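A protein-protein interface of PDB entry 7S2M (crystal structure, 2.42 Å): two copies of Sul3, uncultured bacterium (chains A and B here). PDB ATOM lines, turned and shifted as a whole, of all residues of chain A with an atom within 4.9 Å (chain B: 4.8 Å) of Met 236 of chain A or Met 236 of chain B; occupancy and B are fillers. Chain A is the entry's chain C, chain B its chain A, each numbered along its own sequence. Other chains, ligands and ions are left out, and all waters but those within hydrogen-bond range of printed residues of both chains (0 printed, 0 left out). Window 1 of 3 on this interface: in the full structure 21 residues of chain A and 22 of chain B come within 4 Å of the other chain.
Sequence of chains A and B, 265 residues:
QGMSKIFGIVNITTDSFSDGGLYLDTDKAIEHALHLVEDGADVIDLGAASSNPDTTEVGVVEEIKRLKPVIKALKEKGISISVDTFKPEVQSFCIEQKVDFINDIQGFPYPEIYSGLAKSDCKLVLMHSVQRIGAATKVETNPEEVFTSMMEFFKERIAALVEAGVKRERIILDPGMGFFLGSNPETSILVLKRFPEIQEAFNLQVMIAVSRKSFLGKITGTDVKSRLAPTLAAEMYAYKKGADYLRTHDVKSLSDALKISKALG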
ATOM      1  N   LEU A 232      -0.288 -14.187   8.602  1.00  0.00           N
ATOM      2  CA  LEU A 232       1.098 -14.468   8.962  1.00  0.00           C
ATOM      3  C   LEU A 232       1.190 -15.420  10.147  1.00  0.00           C
ATOM      4  O   LEU A 232       2.084 -16.272  10.198  1.00  0.00           O
ATOM      5  CB  LEU A 232       1.828 -13.163   9.271  1.00  0.00           C
ATOM      6  CG  LEU A 232       2.935 -12.749   8.304  1.00  0.00           C
ATOM      7  CD1 LEU A 232       3.774 -11.645   8.917  1.00  0.00           C
ATOM      8  CD2 LEU A 232       3.797 -13.945   7.934  1.00  0.00           C
ATOM      9  N   ALA A 233       0.281 -15.285  11.116  1.00  0.00           N
ATOM     10  CA  ALA A 233       0.339 -16.126  12.307  1.00  0.00           C
ATOM     11  C   ALA A 233       0.130 -17.595  11.959  1.00  0.00           C
ATOM     12  O   ALA A 233       0.739 -18.479  12.572  1.00  0.00           O
ATOM     13  CB  ALA A 233      -0.698 -15.661  13.328  1.00  0.00           C
ATOM     14  N   ALA A 234      -0.722 -17.877  10.971  1.00  0.00           N
ATOM     15  CA  ALA A 234      -0.991 -19.255  10.584  1.00  0.00           C
ATOM     16  C   ALA A 234       0.110 -19.854   9.718  1.00  0.00           C
ATOM     17  O   ALA A 234       0.262 -21.081   9.696  1.00  0.00           O
ATOM     18  CB  ALA A 234      -2.328 -19.344   9.846  1.00  0.00           C
ATOM     19  N   GLU A 235       0.876 -19.025   9.006  1.00  0.00           N
ATOM     20  CA  GLU A 235       1.968 -19.541   8.187  1.00  0.00           C
ATOM     21  C   GLU A 235       3.195 -19.870   9.030  1.00  0.00           C
ATOM     22  O   GLU A 235       3.912 -20.834   8.735  1.00  0.00           O
ATOM     23  CB  GLU A 235       2.316 -18.537   7.090  1.00  0.00           C
ATOM     24  CG  GLU A 235       1.100 -17.899   6.444  1.00  0.00           C
ATOM     25  CD  GLU A 235       1.458 -16.876   5.385  1.00  0.00           C
ATOM     26  OE1 GLU A 235       2.302 -15.997   5.664  1.00  0.00           O
ATOM     27  OE2 GLU A 235       0.888 -16.949   4.275  1.00  0.00           O
ATOM     28  N   MET A 236       3.458 -19.086  10.078  1.00  0.00           N
ATOM     29  CA  MET A 236       4.533 -19.439  11.000  1.00  0.00           C
ATOM     30  C   MET A 236       4.199 -20.715  11.762  1.00  0.00           C
ATOM     31  O   MET A 236       5.067 -21.575  11.957  1.00  0.00           O
ATOM     32  CB  MET A 236       4.799 -18.289  11.970  1.00  0.00           C
ATOM     33  CG  MET A 236       5.180 -16.979  11.302  1.00  0.00           C
ATOM     34  SD  MET A 236       5.620 -15.707  12.503  1.00  0.00           S
ATOM     35  CE  MET A 236       3.994 -15.128  12.978  1.00  0.00           C
ATOM     36  N   TYR A 237       2.942 -20.854  12.194  1.00  0.00           N
ATOM     37  CA  TYR A 237       2.504 -22.072  12.867  1.00  0.00           C
ATOM     38  C   TYR A 237       2.707 -23.294  11.982  1.00  0.00           C
ATOM     39  O   TYR A 237       3.145 -24.348  12.456  1.00  0.00           O
ATOM     40  CB  TYR A 237       1.035 -21.930  13.272  1.00  0.00           C
ATOM     41  CG  TYR A 237       0.409 -23.161  13.896  1.00  0.00           C
ATOM     42  CD1 TYR A 237      -0.220 -24.122  13.111  1.00  0.00           C
ATOM     43  CD2 TYR A 237       0.428 -23.349  15.271  1.00  0.00           C
ATOM     44  CE1 TYR A 237      -0.801 -25.239  13.681  1.00  0.00           C
ATOM     45  CE2 TYR A 237      -0.150 -24.464  15.848  1.00  0.00           C
ATOM     46  CZ  TYR A 237      -0.763 -25.405  15.049  1.00  0.00           C
ATOM     47  OH  TYR A 237      -1.339 -26.515  15.623  1.00  0.00           O
ATOM     48  N   ALA A 238       2.389 -23.173  10.691  1.00  0.00           N
ATOM     49  CA  ALA A 238       2.598 -24.289   9.774  1.00  0.00           C
ATOM     50  C   ALA A 238       4.081 -24.573   9.582  1.00  0.00           C
ATOM     51  O   ALA A 238       4.489 -25.738   9.496  1.00  0.00           O
ATOM     52  CB  ALA A 238       1.925 -24.000   8.433  1.00  0.00           C
ATOM     53  N   TYR A 239       4.902 -23.522   9.516  1.00  0.00           N
ATOM     54  CA  TYR A 239       6.342 -23.712   9.374  1.00  0.00           C
ATOM     55  C   TYR A 239       6.927 -24.420  10.590  1.00  0.00           C
ATOM     56  O   TYR A 239       7.749 -25.334  10.451  1.00  0.00           O
ATOM     57  CB  TYR A 239       7.029 -22.365   9.156  1.00  0.00           C
ATOM     58  CG  TYR A 239       8.492 -22.346   9.544  1.00  0.00           C
ATOM     59  CD1 TYR A 239       9.457 -22.910   8.720  1.00  0.00           C
ATOM     60  CD2 TYR A 239       8.907 -21.761  10.734  1.00  0.00           C
ATOM     61  CE1 TYR A 239      10.795 -22.895   9.070  1.00  0.00           C
ATOM     62  CE2 TYR A 239      10.245 -21.742  11.094  1.00  0.00           C
ATOM     63  CZ  TYR A 239      11.183 -22.312  10.257  1.00  0.00           C
ATOM     64  OH  TYR A 239      12.513 -22.295  10.608  1.00  0.00           O
ATOM     65  N   LYS A 240       6.508 -24.015  11.790  1.00  0.00           N
ATOM     66  CA  LYS A 240       7.040 -24.593  13.018  1.00  0.00           C
ATOM     67  C   LYS A 240       6.621 -26.042  13.226  1.00  0.00           C
ATOM     68  O   LYS A 240       7.216 -26.722  14.069  1.00  0.00           O
ATOM     69  CB  LYS A 240       6.605 -23.753  14.222  1.00  0.00           C
ATOM     70  CG  LYS A 240       7.225 -22.364  14.269  1.00  0.00           C
ATOM     71  CD  LYS A 240       6.599 -21.514  15.364  1.00  0.00           C
ATOM     72  CE  LYS A 240       7.011 -20.056  15.237  1.00  0.00           C
ATOM     73  NZ  LYS A 240       6.438 -19.217  16.326  1.00  0.00           N
ATOM     74  N   ALA A 257       9.264 -13.310   8.087  1.00  0.00           N
ATOM     75  CA  ALA A 257       8.748 -14.028   9.247  1.00  0.00           C
ATOM     76  C   ALA A 257       9.480 -15.350   9.439  1.00  0.00           C
ATOM     77  O   ALA A 257       9.707 -15.781  10.576  1.00  0.00           O
ATOM     78  CB  ALA A 257       7.245 -14.262   9.101  1.00  0.00           C
ATOM     79  N   LEU A 258       9.870 -15.997   8.340  1.00  0.00           N
ATOM     80  CA  LEU A 258      10.578 -17.267   8.436  1.00  0.00           C
ATOM     81  C   LEU A 258      12.046 -17.075   8.794  1.00  0.00           C
ATOM     82  O   LEU A 258      12.647 -17.959   9.415  1.00  0.00           O
ATOM     83  CB  LEU A 258      10.442 -18.038   7.122  1.00  0.00           C
ATOM     84  CG  LEU A 258       9.057 -18.635   6.849  1.00  0.00           C
ATOM     85  CD1 LEU A 258       9.149 -19.811   5.889  1.00  0.00           C
ATOM     86  CD2 LEU A 258       8.368 -19.055   8.142  1.00  0.00           C
ATOM     87  N   SER A 261      11.912 -16.417  12.581  1.00  0.00           N
ATOM     88  CA  SER A 261      11.499 -17.605  13.321  1.00  0.00           C
ATOM     89  C   SER A 261      12.630 -18.621  13.426  1.00  0.00           C
ATOM     90  O   SER A 261      12.796 -19.266  14.467  1.00  0.00           O
ATOM     91  CB  SER A 261      10.274 -18.233  12.658  1.00  0.00           C
ATOM     92  OG  SER A 261       9.085 -17.565  13.043  1.00  0.00           O
ATOM     93  N   LEU B 232       6.184  -8.710  13.952  1.00  0.00           N
ATOM     94  CA  LEU B 232       5.191  -9.680  14.400  1.00  0.00           C
ATOM     95  C   LEU B 232       5.819 -11.043  14.656  1.00  0.00           C
ATOM     96  O   LEU B 232       5.443 -11.736  15.610  1.00  0.00           O
ATOM     97  CB  LEU B 232       4.070  -9.799  13.369  1.00  0.00           C
ATOM     98  CG  LEU B 232       2.706 -10.234  13.907  1.00  0.00           C
ATOM     99  CD1 LEU B 232       2.077  -9.127  14.739  1.00  0.00           C
ATOM    100  CD2 LEU B 232       1.791 -10.647  12.768  1.00  0.00           C
ATOM    101  N   ALA B 233       6.769 -11.452  13.811  1.00  0.00           N
ATOM    102  CA  ALA B 233       7.410 -12.749  13.994  1.00  0.00           C
ATOM    103  C   ALA B 233       8.151 -12.816  15.323  1.00  0.00           C
ATOM    104  O   ALA B 233       8.093 -13.832  16.025  1.00  0.00           O
ATOM    105  CB  ALA B 233       8.360 -13.036  12.831  1.00  0.00           C
ATOM    106  N   ALA B 234       8.846 -11.736  15.689  1.00  0.00           N
ATOM    107  CA  ALA B 234       9.547 -11.710  16.968  1.00  0.00           C
ATOM    108  C   ALA B 234       8.572 -11.583  18.131  1.00  0.00           C
ATOM    109  O   ALA B 234       8.755 -12.221  19.174  1.00  0.00           O
ATOM    110  CB  ALA B 234      10.561 -10.567  16.989  1.00  0.00           C
ATOM    111  N   GLU B 235       7.533 -10.760  17.973  1.00  0.00           N
ATOM    112  CA  GLU B 235       6.527 -10.633  19.023  1.00  0.00           C
ATOM    113  C   GLU B 235       5.784 -11.943  19.241  1.00  0.00           C
ATOM    114  O   GLU B 235       5.313 -12.214  20.352  1.00  0.00           O
ATOM    115  CB  GLU B 235       5.541  -9.520  18.675  1.00  0.00           C
ATOM    116  CG  GLU B 235       6.031  -8.123  19.006  1.00  0.00           C
ATOM    117  CD  GLU B 235       5.227  -7.053  18.296  1.00  0.00           C
ATOM    118  OE1 GLU B 235       5.444  -5.856  18.581  1.00  0.00           O
ATOM    119  OE2 GLU B 235       4.376  -7.409  17.454  1.00  0.00           O
ATOM    120  N   MET B 236       5.660 -12.762  18.194  1.00  0.00           N
ATOM    121  CA  MET B 236       5.017 -14.064  18.339  1.00  0.00           C
ATOM    122  C   MET B 236       5.865 -15.023  19.161  1.00  0.00           C
ATOM    123  O   MET B 236       5.345 -15.723  20.038  1.00  0.00           O
ATOM    124  CB  MET B 236       4.722 -14.662  16.964  1.00  0.00           C
ATOM    125  CG  MET B 236       3.393 -14.251  16.380  1.00  0.00           C
ATOM    126  SD  MET B 236       2.121 -14.272  17.654  1.00  0.00           S
ATOM    127  CE  MET B 236       0.804 -15.090  16.767  1.00  0.00           C
ATOM    128  N   TYR B 237       7.169 -15.075  18.886  1.00  0.00           N
ATOM    129  CA  TYR B 237       8.044 -15.997  19.603  1.00  0.00           C
ATOM    130  C   TYR B 237       8.051 -15.703  21.099  1.00  0.00           C
ATOM    131  O   TYR B 237       7.977 -16.624  21.922  1.00  0.00           O
ATOM    132  CB  TYR B 237       9.458 -15.920  19.028  1.00  0.00           C
ATOM    133  CG  TYR B 237      10.473 -16.774  19.749  1.00  0.00           C
ATOM    134  CD1 TYR B 237      11.245 -16.252  20.780  1.00  0.00           C
ATOM    135  CD2 TYR B 237      10.659 -18.103  19.399  1.00  0.00           C
ATOM    136  CE1 TYR B 237      12.175 -17.030  21.439  1.00  0.00           C
ATOM    137  CE2 TYR B 237      11.584 -18.889  20.053  1.00  0.00           C
ATOM    138  CZ  TYR B 237      12.339 -18.348  21.072  1.00  0.00           C
ATOM    139  OH  TYR B 237      13.265 -19.129  21.726  1.00  0.00           O
ATOM    140  N   ALA B 238       8.131 -14.424  21.471  1.00  0.00           N
ATOM    141  CA  ALA B 238       8.129 -14.065  22.885  1.00  0.00           C
ATOM    142  C   ALA B 238       6.804 -14.407  23.552  1.00  0.00           C
ATOM    143  O   ALA B 238       6.774 -14.693  24.755  1.00  0.00           O
ATOM    144  CB  ALA B 238       8.440 -12.578  23.053  1.00  0.00           C
ATOM    145  N   TYR B 239       5.702 -14.382  22.800  1.00  0.00           N
ATOM    146  CA  TYR B 239       4.410 -14.740  23.374  1.00  0.00           C
ATOM    147  C   TYR B 239       4.359 -16.221  23.726  1.00  0.00           C
ATOM    148  O   TYR B 239       3.960 -16.594  24.835  1.00  0.00           O
ATOM    149  CB  TYR B 239       3.284 -14.381  22.407  1.00  0.00           C
ATOM    150  CG  TYR B 239       1.934 -14.909  22.837  1.00  0.00           C
ATOM    151  CD1 TYR B 239       1.317 -14.434  23.985  1.00  0.00           C
ATOM    152  CD2 TYR B 239       1.281 -15.889  22.099  1.00  0.00           C
ATOM    153  CE1 TYR B 239       0.085 -14.914  24.387  1.00  0.00           C
ATOM    154  CE2 TYR B 239       0.048 -16.375  22.491  1.00  0.00           C
ATOM    155  CZ  TYR B 239      -0.545 -15.885  23.636  1.00  0.00           C
ATOM    156  OH  TYR B 239      -1.772 -16.365  24.032  1.00  0.00           O
ATOM    157  N   LYS B 240       4.761 -17.082  22.787  1.00  0.00           N
ATOM    158  CA  LYS B 240       4.781 -18.516  23.045  1.00  0.00           C
ATOM    159  C   LYS B 240       5.805 -18.897  24.102  1.00  0.00           C
ATOM    160  O   LYS B 240       5.674 -19.959  24.720  1.00  0.00           O
ATOM    161  CB  LYS B 240       5.059 -19.280  21.748  1.00  0.00           C
ATOM    162  CG  LYS B 240       4.380 -18.694  20.516  1.00  0.00           C
ATOM    163  CD  LYS B 240       2.863 -18.776  20.616  1.00  0.00           C
ATOM    164  CE  LYS B 240       2.342 -20.139  20.176  1.00  0.00           C
ATOM    165  NZ  LYS B 240       1.794 -20.121  18.787  1.00  0.00           N
ATOM    166  N   ALA B 257      -3.122 -11.440  15.753  1.00  0.00           N
ATOM    167  CA  ALA B 257      -2.209 -12.575  15.687  1.00  0.00           C
ATOM    168  C   ALA B 257      -2.347 -13.466  16.916  1.00  0.00           C
ATOM    169  O   ALA B 257      -2.332 -14.698  16.802  1.00  0.00           O
ATOM    170  CB  ALA B 257      -0.770 -12.083  15.534  1.00  0.00           C
ATOM    171  N   LEU B 258      -2.486 -12.861  18.100  1.00  0.00           N
ATOM    172  CA  LEU B 258      -2.672 -13.647  19.316  1.00  0.00           C
ATOM    173  C   LEU B 258      -3.965 -14.446  19.276  1.00  0.00           C
ATOM    174  O   LEU B 258      -4.061 -15.504  19.911  1.00  0.00           O
ATOM    175  CB  LEU B 258      -2.661 -12.735  20.543  1.00  0.00           C
ATOM    176  CG  LEU B 258      -1.333 -12.076  20.914  1.00  0.00           C
ATOM    177  CD1 LEU B 258      -1.344 -11.624  22.368  1.00  0.00           C
ATOM    178  CD2 LEU B 258      -0.167 -13.012  20.643  1.00  0.00           C
ATOM    179  N   SER B 261      -3.094 -17.806  17.286  1.00  0.00           N
ATOM    180  CA  SER B 261      -2.318 -18.789  18.035  1.00  0.00           C
ATOM    181  C   SER B 261      -3.125 -19.399  19.173  1.00  0.00           C
ATOM    182  O   SER B 261      -2.889 -20.553  19.548  1.00  0.00           O
ATOM    183  CB  SER B 261      -1.040 -18.147  18.576  1.00  0.00           C
ATOM    184  OG  SER B 261       0.056 -18.394  17.713  1.00  0.00           O
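CB of Ala 233 of chain A touches CE of Met 236 of chain B (3.8 Å). Ala 257 of chain B touches Ala 233 of chain A. Met 236 of chain A touches Ala 233 of chain B. CG of Met 236 of chain B touches CE of Met 236 of chain A, at 3.6 Å. CA of Ala 257 of chain A touches CB of Ala 233 of chain B (3.7 Å).
The side-chain hydroxyl (OG) of Ser 261 of chain A is in hydrogen-bond range of the backbone carbonyl oxygen (O) of Ala 257 of chain A (3.1 Å).
Of chain B, only Ala 233 and Met 236 come within 4 Å of Met 236 of chain A. Of chain A, only Ala 233 (3.8 Å) and Met 236 (3.6 Å) come within 4 Å of Met 236 of chain B. Printed residues of chain A within 4 Å of Ala 257 of chain B: Ala 233. Of the printed residues of chain A, Ala 233 of chain B touches Met 236 and Ala 257. Printed residues of chain B within 4 Å of Ala 233 of chain A: Met 236 (3.8 Å) and Ala 257 (3.96 Å). Of the printed residues of chain B, Ala 257 of chain A touches Ala 233. Tyr 237 of chain A touches none of the printed residues of chain B. The nearest printed residue of chain A that does not touch Met 236 of chain B is Lys 240 of chain A (4.9 Å).
Ala 233 of chain A touches Met 236 of chain B, and with the chains exchanged Met 236 of chain A touches Ala 233 of chain B. Ala 233 of chain A touches Ala 257 of chain B, and with the chains exchanged Ala 257 of chain A touches Ala 233 of chain B. Met 236 of chain B touches its own counterpart, Met 236 of chain A. Positions printed for both chains: 232, 233, 234, 235, 236, 237, 238, 239, 240, 257, 258 and 261. Of the 5 pairs that touch across the chains among the printed residues, 5 have their exchanged pair printed and touching as well.
Of the 12 printed residues of chain A, 3 touch a printed residue of chain B. Hydrophobic or aromatic side chains of chain A that line the printed part of chain B: Ala 233 and Met 236. Printed residues of chain B that touch a printed residue of chain A: Ala 233, Met 236 and Ala 257. Hydrophobic or aromatic side chains of chain B that line the printed part of chain A: Ala 233 and Met 236. Along chain B the printed residues that touch a printed residue of chain A span positions 233 to 257. Among the printed residues, no Asp or Glu carboxylate lies within 4 Å of a Lys or Arg side-chain nitrogen of the other chain.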
